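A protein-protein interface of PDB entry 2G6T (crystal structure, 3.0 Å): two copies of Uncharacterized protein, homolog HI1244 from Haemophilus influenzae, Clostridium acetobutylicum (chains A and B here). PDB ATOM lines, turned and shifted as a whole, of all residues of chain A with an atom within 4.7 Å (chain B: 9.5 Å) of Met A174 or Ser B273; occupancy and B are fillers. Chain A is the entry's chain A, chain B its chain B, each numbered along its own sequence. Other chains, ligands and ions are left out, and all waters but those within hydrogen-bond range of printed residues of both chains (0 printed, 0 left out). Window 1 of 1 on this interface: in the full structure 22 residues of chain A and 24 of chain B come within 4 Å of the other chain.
O of Cys A172 lies close to OG of Ser B273 (3.4 Å). ND2 of Asn B272 is in hydrogen-bond range of O of Phe A190. N of Asn B272 sits at hydrogen-bond distance from O of Asn A191. The side-chain sulfur (SG) of Cys A172 is in hydrogen-bond range of the side-chain hydroxyl (OH) of Tyr B259 (3.8 Å).
The side-chain sulfur (SG) of Cys B263 lies close to the side-chain hydroxyl (OH) of Tyr B259. N of Phe A190 is in hydrogen-bond range of O of Pro A175, at 3.2 Å. The side-chain amino group (NZ) of Lys B222 lies within hydrogen-bond range of the backbone carbonyl oxygen (O) of Ser B273, at 3.4 Å. The side-chain hydroxyl of Ser B271 lies within hydrogen-bond range of the backbone NH of Ser B273 (3.0 Å). The side-chain hydroxyl (OH) of Tyr B259 is in hydrogen-bond range of the backbone NH (N) of Asn B274 (3.2 Å). The side-chain amide oxygen (OD1) of Asn B272 is in hydrogen-bond range of the side-chain hydroxyl (OG) of Ser B273 (3.1 Å).
Among the printed residues, merely in contact across the chains: Cys A172 with Lys B222 (3.8 Å), Cys A172 with Pro B245 (3.5 Å), Met A174 with Asn B272 (3.4 Å), Met A174 with Ser B273 (3.6 Å), Pro A175 with Asn B272 (3.6 Å), Asn A191 with Thr B270 (3.6 Å) and Asn A191 with Ser B271 (3.1 Å).
Met A174 touches just these residues of chain B: Asn B272 (3.4 Å) and Ser B273 (3.6 Å). Of chain A, only Cys A172 and Met A174 come within 4 Å of Ser B273. Of chain B, only Lys B222, Pro B245, Tyr B259 and Ser B273 come within 4 Å of Cys A172. No residue of chain B comes within 4 Å of Thr A173. Of chain B, only Asn B272 (3.6 Å) comes within 4 Å of Pro A175. Printed residues of chain A within 4 Å of Ser B271: Asn A191. Printed residues of chain B within 4 Å of Asn A191: Thr B270 (3.6 Å), Ser B271 (3.1 Å) and Asn B272 (3.0 Å). Of the printed residues of chain A, Pro B245 touches Cys A172 (3.5 Å). Printed residues of chain A within 4 Å of Lys B222: Cys A172. Printed residues of chain A within 4 Å of Thr B270: Asn A191. Arg B262 touches none of the printed residues of chain A. The nearest residue of chain B that does not touch Met A174 is Ser B271 (4.4 Å). The nearest printed residue of chain A that does not touch Asn B272 is Thr A173 (5.4 Å).
Hydrophobic or aromatic side chains of chain B within 4 Å of the printed part of chain A: Pro B245 and Tyr B259. Hydrophobic or aromatic side chains of chain A within 4 Å of the printed part of chain B: Met A174 and Pro A175. Among the printed residues, no Asp or Glu carboxylate lies within 4 Å of a Lys or Arg side-chain nitrogen of the other chain.
No position is printed for both chains.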
ATOM      1  N   TYR A 140     -24.422  21.559  40.008  1.00  0.00           N
ATOM      2  CA  TYR A 140     -24.991  20.797  41.102  1.00  0.00           C
ATOM      3  C   TYR A 140     -23.924  20.394  42.113  1.00  0.00           C
ATOM      4  O   TYR A 140     -22.747  20.275  41.776  1.00  0.00           O
ATOM      5  CB  TYR A 140     -25.706  19.557  40.560  1.00  0.00           C
ATOM      6  CG  TYR A 140     -24.797  18.530  39.930  1.00  0.00           C
ATOM      7  CD1 TYR A 140     -24.260  17.487  40.685  1.00  0.00           C
ATOM      8  CD2 TYR A 140     -24.451  18.611  38.584  1.00  0.00           C
ATOM      9  CE1 TYR A 140     -23.402  16.549  40.112  1.00  0.00           C
ATOM     10  CE2 TYR A 140     -23.593  17.681  38.000  1.00  0.00           C
ATOM     11  CZ  TYR A 140     -23.077  16.656  38.769  1.00  0.00           C
ATOM     12  OH  TYR A 140     -22.242  15.730  38.196  1.00  0.00           O
ATOM     13  N   GLN A 165     -11.152  20.883  38.353  1.00  0.00           N
ATOM     14  CA  GLN A 165     -11.126  20.184  37.068  1.00  0.00           C
ATOM     15  C   GLN A 165     -11.399  21.195  35.962  1.00  0.00           C
ATOM     16  O   GLN A 165     -12.316  22.002  36.075  1.00  0.00           O
ATOM     17  CB  GLN A 165     -12.182  19.092  37.046  1.00  0.00           C
ATOM     18  CG  GLN A 165     -12.276  18.343  35.741  1.00  0.00           C
ATOM     19  CD  GLN A 165     -13.040  17.048  35.906  1.00  0.00           C
ATOM     20  OE1 GLN A 165     -12.531  16.084  36.483  1.00  0.00           O
ATOM     21  NE2 GLN A 165     -14.277  17.026  35.424  1.00  0.00           N
ATOM     22  N   GLY A 167     -12.268  20.534  32.713  1.00  0.00           N
ATOM     23  CA  GLY A 167     -13.308  20.163  31.767  1.00  0.00           C
ATOM     24  C   GLY A 167     -12.922  20.167  30.298  1.00  0.00           C
ATOM     25  O   GLY A 167     -12.372  21.135  29.783  1.00  0.00           O
ATOM     26  N   CYS A 172     -16.344  14.370  27.390  1.00  0.00           N
ATOM     27  CA  CYS A 172     -17.551  14.751  28.102  1.00  0.00           C
ATOM     28  C   CYS A 172     -17.243  15.127  29.544  1.00  0.00           C
ATOM     29  O   CYS A 172     -18.025  14.854  30.446  1.00  0.00           O
ATOM     30  CB  CYS A 172     -18.578  13.616  28.054  1.00  0.00           C
ATOM     31  SG  CYS A 172     -19.239  13.287  26.400  1.00  0.00           S
ATOM     32  N   THR A 173     -16.094  15.761  29.747  1.00  0.00           N
ATOM     33  CA  THR A 173     -15.670  16.192  31.071  1.00  0.00           C
ATOM     34  C   THR A 173     -16.100  17.627  31.314  1.00  0.00           C
ATOM     35  O   THR A 173     -15.736  18.527  30.563  1.00  0.00           O
ATOM     36  CB  THR A 173     -14.153  16.114  31.205  1.00  0.00           C
ATOM     37  OG1 THR A 173     -13.737  14.758  31.018  1.00  0.00           O
ATOM     38  CG2 THR A 173     -13.711  16.601  32.566  1.00  0.00           C
ATOM     39  N   MET A 174     -16.878  17.835  32.369  1.00  0.00           N
ATOM     40  CA  MET A 174     -17.362  19.166  32.705  1.00  0.00           C
ATOM     41  C   MET A 174     -16.451  19.864  33.701  1.00  0.00           C
ATOM     42  O   MET A 174     -15.832  19.225  34.555  1.00  0.00           O
ATOM     43  CB  MET A 174     -18.766  19.082  33.286  1.00  0.00           C
ATOM     44  CG  MET A 174     -18.868  18.143  34.465  1.00  0.00           C
ATOM     45  SD  MET A 174     -20.637  18.123  35.232  1.00  0.00           S
ATOM     46  CE  MET A 174     -21.629  17.611  33.647  1.00  0.00           C
ATOM     47  N   PRO A 175     -16.356  21.194  33.601  1.00  0.00           N
ATOM     48  CA  PRO A 175     -15.519  21.991  34.497  1.00  0.00           C
ATOM     49  C   PRO A 175     -16.033  21.904  35.928  1.00  0.00           C
ATOM     50  O   PRO A 175     -17.207  22.175  36.172  1.00  0.00           O
ATOM     51  CB  PRO A 175     -15.662  23.407  33.934  1.00  0.00           C
ATOM     52  CG  PRO A 175     -15.948  23.172  32.479  1.00  0.00           C
ATOM     53  CD  PRO A 175     -16.932  22.039  32.541  1.00  0.00           C
ATOM     54  N   LYS A 176     -15.174  21.519  36.868  1.00  0.00           N
ATOM     55  CA  LYS A 176     -15.582  21.444  38.266  1.00  0.00           C
ATOM     56  C   LYS A 176     -14.920  22.544  39.068  1.00  0.00           C
ATOM     57  O   LYS A 176     -13.853  23.031  38.710  1.00  0.00           O
ATOM     58  CB  LYS A 176     -15.236  20.093  38.867  1.00  0.00           C
ATOM     59  CG  LYS A 176     -16.137  18.989  38.393  1.00  0.00           C
ATOM     60  CD  LYS A 176     -15.840  17.693  39.111  1.00  0.00           C
ATOM     61  CE  LYS A 176     -16.742  16.604  38.600  1.00  0.00           C
ATOM     62  NZ  LYS A 176     -16.668  16.578  37.111  1.00  0.00           N
ATOM     63  N   ASN A 189     -20.141  21.149  40.543  1.00  0.00           N
ATOM     64  CA  ASN A 189     -20.053  20.518  39.238  1.00  0.00           C
ATOM     65  C   ASN A 189     -20.802  21.355  38.202  1.00  0.00           C
ATOM     66  O   ASN A 189     -22.002  21.190  38.017  1.00  0.00           O
ATOM     67  CB  ASN A 189     -20.636  19.105  39.298  1.00  0.00           C
ATOM     68  CG  ASN A 189     -20.126  18.310  40.492  1.00  0.00           C
ATOM     69  OD1 ASN A 189     -20.576  18.510  41.615  1.00  0.00           O
ATOM     70  ND2 ASN A 189     -19.177  17.409  40.252  1.00  0.00           N
ATOM     71  N   PHE A 190     -20.090  22.255  37.531  1.00  0.00           N
ATOM     72  CA  PHE A 190     -20.706  23.118  36.524  1.00  0.00           C
ATOM     73  C   PHE A 190     -20.978  22.314  35.273  1.00  0.00           C
ATOM     74  O   PHE A 190     -20.048  21.832  34.644  1.00  0.00           O
ATOM     75  CB  PHE A 190     -19.777  24.283  36.166  1.00  0.00           C
ATOM     76  CG  PHE A 190     -19.233  25.018  37.360  1.00  0.00           C
ATOM     77  CD1 PHE A 190     -17.895  24.896  37.713  1.00  0.00           C
ATOM     78  CD2 PHE A 190     -20.061  25.808  38.146  1.00  0.00           C
ATOM     79  CE1 PHE A 190     -17.397  25.548  38.833  1.00  0.00           C
ATOM     80  CE2 PHE A 190     -19.569  26.461  39.262  1.00  0.00           C
ATOM     81  CZ  PHE A 190     -18.237  26.331  39.608  1.00  0.00           C
ATOM     82  N   ASN A 191     -22.240  22.186  34.886  1.00  0.00           N
ATOM     83  CA  ASN A 191     -22.543  21.396  33.700  1.00  0.00           C
ATOM     84  C   ASN A 191     -23.168  22.183  32.555  1.00  0.00           C
ATOM     85  O   ASN A 191     -23.895  21.628  31.734  1.00  0.00           O
ATOM     86  CB  ASN A 191     -23.453  20.228  34.081  1.00  0.00           C
ATOM     87  CG  ASN A 191     -24.875  20.663  34.333  1.00  0.00           C
ATOM     88  OD1 ASN A 191     -25.125  21.612  35.078  1.00  0.00           O
ATOM     89  ND2 ASN A 191     -25.820  19.969  33.711  1.00  0.00           N
ATOM     90  N   LEU B 220     -22.265   3.682  22.995  1.00  0.00           N
ATOM     91  CA  LEU B 220     -21.871   5.049  23.248  1.00  0.00           C
ATOM     92  C   LEU B 220     -20.772   5.100  24.291  1.00  0.00           C
ATOM     93  O   LEU B 220     -21.011   4.790  25.457  1.00  0.00           O
ATOM     94  CB  LEU B 220     -23.063   5.854  23.743  1.00  0.00           C
ATOM     95  CG  LEU B 220     -22.746   7.154  24.485  1.00  0.00           C
ATOM     96  CD1 LEU B 220     -21.957   8.108  23.594  1.00  0.00           C
ATOM     97  CD2 LEU B 220     -24.054   7.785  24.923  1.00  0.00           C
ATOM     98  N   LYS B 222     -18.507   7.658  26.069  1.00  0.00           N
ATOM     99  CA  LYS B 222     -18.344   9.086  26.293  1.00  0.00           C
ATOM    100  C   LYS B 222     -16.942   9.517  26.664  1.00  0.00           C
ATOM    101  O   LYS B 222     -16.409  10.469  26.106  1.00  0.00           O
ATOM    102  CB  LYS B 222     -19.305   9.566  27.379  1.00  0.00           C
ATOM    103  CG  LYS B 222     -20.742   9.169  27.145  1.00  0.00           C
ATOM    104  CD  LYS B 222     -21.702  10.260  27.603  1.00  0.00           C
ATOM    105  CE  LYS B 222     -21.550  10.592  29.083  1.00  0.00           C
ATOM    106  NZ  LYS B 222     -22.498  11.674  29.505  1.00  0.00           N
ATOM    107  N   ASP B 223     -16.342   8.821  27.615  1.00  0.00           N
ATOM    108  CA  ASP B 223     -15.011   9.175  28.071  1.00  0.00           C
ATOM    109  C   ASP B 223     -13.889   8.747  27.149  1.00  0.00           C
ATOM    110  O   ASP B 223     -14.105   8.126  26.111  1.00  0.00           O
ATOM    111  CB  ASP B 223     -14.768   8.582  29.450  1.00  0.00           C
ATOM    112  CG  ASP B 223     -15.011   7.094  29.482  1.00  0.00           C
ATOM    113  OD1 ASP B 223     -14.328   6.362  28.723  1.00  0.00           O
ATOM    114  OD2 ASP B 223     -15.891   6.663  30.262  1.00  0.00           O
ATOM    115  N   PRO B 245     -17.203  11.324  21.487  1.00  0.00           N
ATOM    116  CA  PRO B 245     -16.993  12.779  21.566  1.00  0.00           C
ATOM    117  C   PRO B 245     -15.930  13.362  20.633  1.00  0.00           C
ATOM    118  O   PRO B 245     -15.840  14.574  20.481  1.00  0.00           O
ATOM    119  CB  PRO B 245     -16.618  12.997  23.029  1.00  0.00           C
ATOM    120  CG  PRO B 245     -17.369  11.935  23.716  1.00  0.00           C
ATOM    121  CD  PRO B 245     -17.098  10.736  22.832  1.00  0.00           C
ATOM    122  N   TYR B 259     -22.375  18.420  17.585  1.00  0.00           N
ATOM    123  CA  TYR B 259     -22.502  18.129  19.011  1.00  0.00           C
ATOM    124  C   TYR B 259     -21.528  18.988  19.813  1.00  0.00           C
ATOM    125  O   TYR B 259     -21.928  19.696  20.740  1.00  0.00           O
ATOM    126  CB  TYR B 259     -22.235  16.646  19.296  1.00  0.00           C
ATOM    127  CG  TYR B 259     -21.982  16.376  20.754  1.00  0.00           C
ATOM    128  CD1 TYR B 259     -20.698  16.141  21.225  1.00  0.00           C
ATOM    129  CD2 TYR B 259     -23.011  16.466  21.676  1.00  0.00           C
ATOM    130  CE1 TYR B 259     -20.443  16.015  22.588  1.00  0.00           C
ATOM    131  CE2 TYR B 259     -22.772  16.343  23.039  1.00  0.00           C
ATOM    132  CZ  TYR B 259     -21.488  16.124  23.492  1.00  0.00           C
ATOM    133  OH  TYR B 259     -21.254  16.067  24.850  1.00  0.00           O
ATOM    134  N   ILE B 260     -20.246  18.912  19.459  1.00  0.00           N
ATOM    135  CA  ILE B 260     -19.223  19.702  20.134  1.00  0.00           C
ATOM    136  C   ILE B 260     -19.626  21.168  20.037  1.00  0.00           C
ATOM    137  O   ILE B 260     -19.453  21.937  20.983  1.00  0.00           O
ATOM    138  CB  ILE B 260     -17.853  19.515  19.472  1.00  0.00           C
ATOM    139  CG1 ILE B 260     -17.438  18.044  19.563  1.00  0.00           C
ATOM    140  CG2 ILE B 260     -16.829  20.426  20.130  1.00  0.00           C
ATOM    141  CD1 ILE B 260     -17.350  17.519  20.977  1.00  0.00           C
ATOM    142  N   ARG B 262     -22.736  22.418  19.756  1.00  0.00           N
ATOM    143  CA  ARG B 262     -23.822  22.616  20.702  1.00  0.00           C
ATOM    144  C   ARG B 262     -23.273  22.751  22.112  1.00  0.00           C
ATOM    145  O   ARG B 262     -23.728  23.596  22.879  1.00  0.00           O
ATOM    146  CB  ARG B 262     -24.810  21.448  20.641  1.00  0.00           C
ATOM    147  CG  ARG B 262     -26.104  21.726  21.392  1.00  0.00           C
ATOM    148  CD  ARG B 262     -27.032  20.521  21.468  1.00  0.00           C
ATOM    149  NE  ARG B 262     -26.559  19.497  22.395  1.00  0.00           N
ATOM    150  CZ  ARG B 262     -27.329  18.531  22.892  1.00  0.00           C
ATOM    151  NH1 ARG B 262     -28.605  18.461  22.549  1.00  0.00           N
ATOM    152  NH2 ARG B 262     -26.829  17.634  23.736  1.00  0.00           N
ATOM    153  N   CYS B 263     -22.287  21.924  22.445  1.00  0.00           N
ATOM    154  CA  CYS B 263     -21.681  21.951  23.773  1.00  0.00           C
ATOM    155  C   CYS B 263     -21.116  23.306  24.148  1.00  0.00           C
ATOM    156  O   CYS B 263     -21.509  23.895  25.150  1.00  0.00           O
ATOM    157  CB  CYS B 263     -20.563  20.915  23.885  1.00  0.00           C
ATOM    158  SG  CYS B 263     -21.128  19.238  24.181  1.00  0.00           S
ATOM    159  N   ILE B 264     -20.194  23.806  23.341  1.00  0.00           N
ATOM    160  CA  ILE B 264     -19.573  25.081  23.646  1.00  0.00           C
ATOM    161  C   ILE B 264     -20.302  26.310  23.109  1.00  0.00           C
ATOM    162  O   ILE B 264     -19.900  27.432  23.388  1.00  0.00           O
ATOM    163  CB  ILE B 264     -18.107  25.102  23.143  1.00  0.00           C
ATOM    164  CG1 ILE B 264     -18.076  25.024  21.618  1.00  0.00           C
ATOM    165  CG2 ILE B 264     -17.335  23.928  23.740  1.00  0.00           C
ATOM    166  CD1 ILE B 264     -16.721  24.659  21.041  1.00  0.00           C
ATOM    167  N   ARG B 269     -28.641  25.051  25.801  1.00  0.00           N
ATOM    168  CA  ARG B 269     -28.152  23.703  26.081  1.00  0.00           C
ATOM    169  C   ARG B 269     -28.405  23.357  27.540  1.00  0.00           C
ATOM    170  O   ARG B 269     -28.327  24.221  28.412  1.00  0.00           O
ATOM    171  CB  ARG B 269     -26.655  23.575  25.786  1.00  0.00           C
ATOM    172  CG  ARG B 269     -25.776  24.425  26.669  1.00  0.00           C
ATOM    173  CD  ARG B 269     -24.333  23.988  26.586  1.00  0.00           C
ATOM    174  NE  ARG B 269     -23.471  24.960  27.242  1.00  0.00           N
ATOM    175  CZ  ARG B 269     -23.081  26.102  26.684  1.00  0.00           C
ATOM    176  NH1 ARG B 269     -23.468  26.407  25.454  1.00  0.00           N
ATOM    177  NH2 ARG B 269     -22.320  26.952  27.362  1.00  0.00           N
ATOM    178  N   THR B 270     -28.717  22.088  27.790  1.00  0.00           N
ATOM    179  CA  THR B 270     -28.993  21.588  29.137  1.00  0.00           C
ATOM    180  C   THR B 270     -27.669  21.289  29.828  1.00  0.00           C
ATOM    181  O   THR B 270     -27.413  21.735  30.947  1.00  0.00           O
ATOM    182  CB  THR B 270     -29.810  20.268  29.081  1.00  0.00           C
ATOM    183  OG1 THR B 270     -31.000  20.475  28.315  1.00  0.00           O
ATOM    184  CG2 THR B 270     -30.192  19.801  30.476  1.00  0.00           C
ATOM    185  N   SER B 271     -26.836  20.525  29.129  1.00  0.00           N
ATOM    186  CA  SER B 271     -25.532  20.110  29.624  1.00  0.00           C
ATOM    187  C   SER B 271     -24.437  20.542  28.649  1.00  0.00           C
ATOM    188  O   SER B 271     -24.719  20.951  27.520  1.00  0.00           O
ATOM    189  CB  SER B 271     -25.520  18.579  29.797  1.00  0.00           C
ATOM    190  OG  SER B 271     -24.242  18.083  30.153  1.00  0.00           O
ATOM    191  N   ASN B 272     -23.192  20.458  29.106  1.00  0.00           N
ATOM    192  CA  ASN B 272     -22.031  20.812  28.296  1.00  0.00           C
ATOM    193  C   ASN B 272     -21.316  19.523  27.928  1.00  0.00           C
ATOM    194  O   ASN B 272     -20.188  19.539  27.433  1.00  0.00           O
ATOM    195  CB  ASN B 272     -21.071  21.722  29.081  1.00  0.00           C
ATOM    196  CG  ASN B 272     -20.767  21.197  30.481  1.00  0.00           C
ATOM    197  OD1 ASN B 272     -20.897  20.002  30.755  1.00  0.00           O
ATOM    198  ND2 ASN B 272     -20.349  22.091  31.369  1.00  0.00           N
ATOM    199  N   SER B 273     -21.983  18.400  28.171  1.00  0.00           N
ATOM    200  CA  SER B 273     -21.391  17.102  27.877  1.00  0.00           C
ATOM    201  C   SER B 273     -22.388  15.944  27.951  1.00  0.00           C
ATOM    202  O   SER B 273     -22.177  14.990  28.701  1.00  0.00           O
ATOM    203  CB  SER B 273     -20.232  16.849  28.846  1.00  0.00           C
ATOM    204  OG  SER B 273     -20.675  16.958  30.190  1.00  0.00           O
ATOM    205  N   ASN B 274     -23.468  16.021  27.177  1.00  0.00           N
ATOM    206  CA  ASN B 274     -24.458  14.953  27.182  1.00  0.00           C
ATOM    207  C   ASN B 274     -24.643  14.311  25.812  1.00  0.00           C
ATOM    208  O   ASN B 274     -25.685  14.439  25.179  1.00  0.00           O
ATOM    209  CB  ASN B 274     -25.800  15.466  27.734  1.00  0.00           C
ATOM    210  CG  ASN B 274     -26.237  16.796  27.121  1.00  0.00           C
ATOM    211  OD1 ASN B 274     -25.487  17.438  26.389  1.00  0.00           O
ATOM    212  ND2 ASN B 274     -27.460  17.214  27.433  1.00  0.00           N
ATOM    213  N   LEU B 275     -23.610  13.610  25.361  1.00  0.00           N
ATOM    214  CA  LEU B 275     -23.649  12.936  24.071  1.00  0.00           C
ATOM    215  C   LEU B 275     -24.816  11.964  23.995  1.00  0.00           C
ATOM    216  O   LEU B 275     -25.345  11.706  22.919  1.00  0.00           O
ATOM    217  CB  LEU B 275     -22.358  12.161  23.827  1.00  0.00           C
ATOM    218  CG  LEU B 275     -21.750  12.336  22.439  1.00  0.00           C
ATOM    219  CD1 LEU B 275     -20.841  11.162  22.177  1.00  0.00           C
ATOM    220  CD2 LEU B 275     -22.821  12.422  21.368  1.00  0.00           C
ATOM    221  N   GLU B 276     -25.206  11.413  25.140  1.00  0.00           N
ATOM    222  CA  GLU B 276     -26.314  10.473  25.181  1.00  0.00           C
ATOM    223  C   GLU B 276     -27.609  11.190  24.810  1.00  0.00           C
ATOM    224  O   GLU B 276     -28.348  10.743  23.933  1.00  0.00           O
ATOM    225  CB  GLU B 276     -26.436   9.852  26.570  1.00  0.00           C
ATOM    226  CG  GLU B 276     -26.871  10.826  27.655  1.00  0.00           C
ATOM    227  CD  GLU B 276     -25.755  11.739  28.138  1.00  0.00           C
ATOM    228  OE1 GLU B 276     -26.048  12.664  28.937  1.00  0.00           O
ATOM    229  OE2 GLU B 276     -24.588  11.527  27.730  1.00  0.00           O
ATOM    230  N   GLN B 277     -27.880  12.313  25.466  1.00  0.00           N
ATOM    231  CA  GLN B 277     -29.091  13.075  25.170  1.00  0.00           C
ATOM    232  C   GLN B 277     -29.092  13.493  23.705  1.00  0.00           C
ATOM    233  O   GLN B 277     -30.117  13.440  23.033  1.00  0.00           O
ATOM    234  CB  GLN B 277     -29.174  14.319  26.060  1.00  0.00           C
ATOM    235  CG  GLN B 277     -29.120  15.649  25.314  1.00  0.00           C
ATOM    236  CD  GLN B 277     -30.433  16.018  24.625  1.00  0.00           C
ATOM    237  OE1 GLN B 277     -31.499  15.970  25.238  1.00  0.00           O
ATOM    238  NE2 GLN B 277     -30.354  16.408  23.354  1.00  0.00           N
ATOM    239  N   TYR B 278     -27.933  13.908  23.214  1.00  0.00           N
ATOM    240  CA  TYR B 278     -27.820  14.342  21.838  1.00  0.00           C
ATOM    241  C   TYR B 278     -28.127  13.221  20.870  1.00  0.00           C
ATOM    242  O   TYR B 278     -28.995  13.362  20.014  1.00  0.00           O
ATOM    243  CB  TYR B 278     -26.420  14.865  21.565  1.00  0.00           C
ATOM    244  CG  TYR B 278     -26.244  15.414  20.166  1.00  0.00           C
ATOM    245  CD1 TYR B 278     -26.081  16.779  19.950  1.00  0.00           C
ATOM    246  CD2 TYR B 278     -26.244  14.568  19.059  1.00  0.00           C
ATOM    247  CE1 TYR B 278     -25.923  17.290  18.670  1.00  0.00           C
ATOM    248  CE2 TYR B 278     -26.090  15.070  17.774  1.00  0.00           C
ATOM    249  CZ  TYR B 278     -25.931  16.432  17.585  1.00  0.00           C
ATOM    250  OH  TYR B 278     -25.800  16.936  16.316  1.00  0.00           O
ATOM    251  N   THR B 279     -27.404  12.115  21.000  1.00  0.00           N
ATOM    252  CA  THR B 279     -27.593  10.976  20.109  1.00  0.00           C
ATOM    253  C   THR B 279     -28.997  10.403  20.132  1.00  0.00           C
ATOM    254  O   THR B 279     -29.455   9.862  19.137  1.00  0.00           O
ATOM    255  CB  THR B 279     -26.609   9.830  20.424  1.00  0.00           C
ATOM    256  OG1 THR B 279     -26.567   9.600  21.836  1.00  0.00           O
ATOM    257  CG2 THR B 279     -25.223  10.168  19.933  1.00  0.00           C
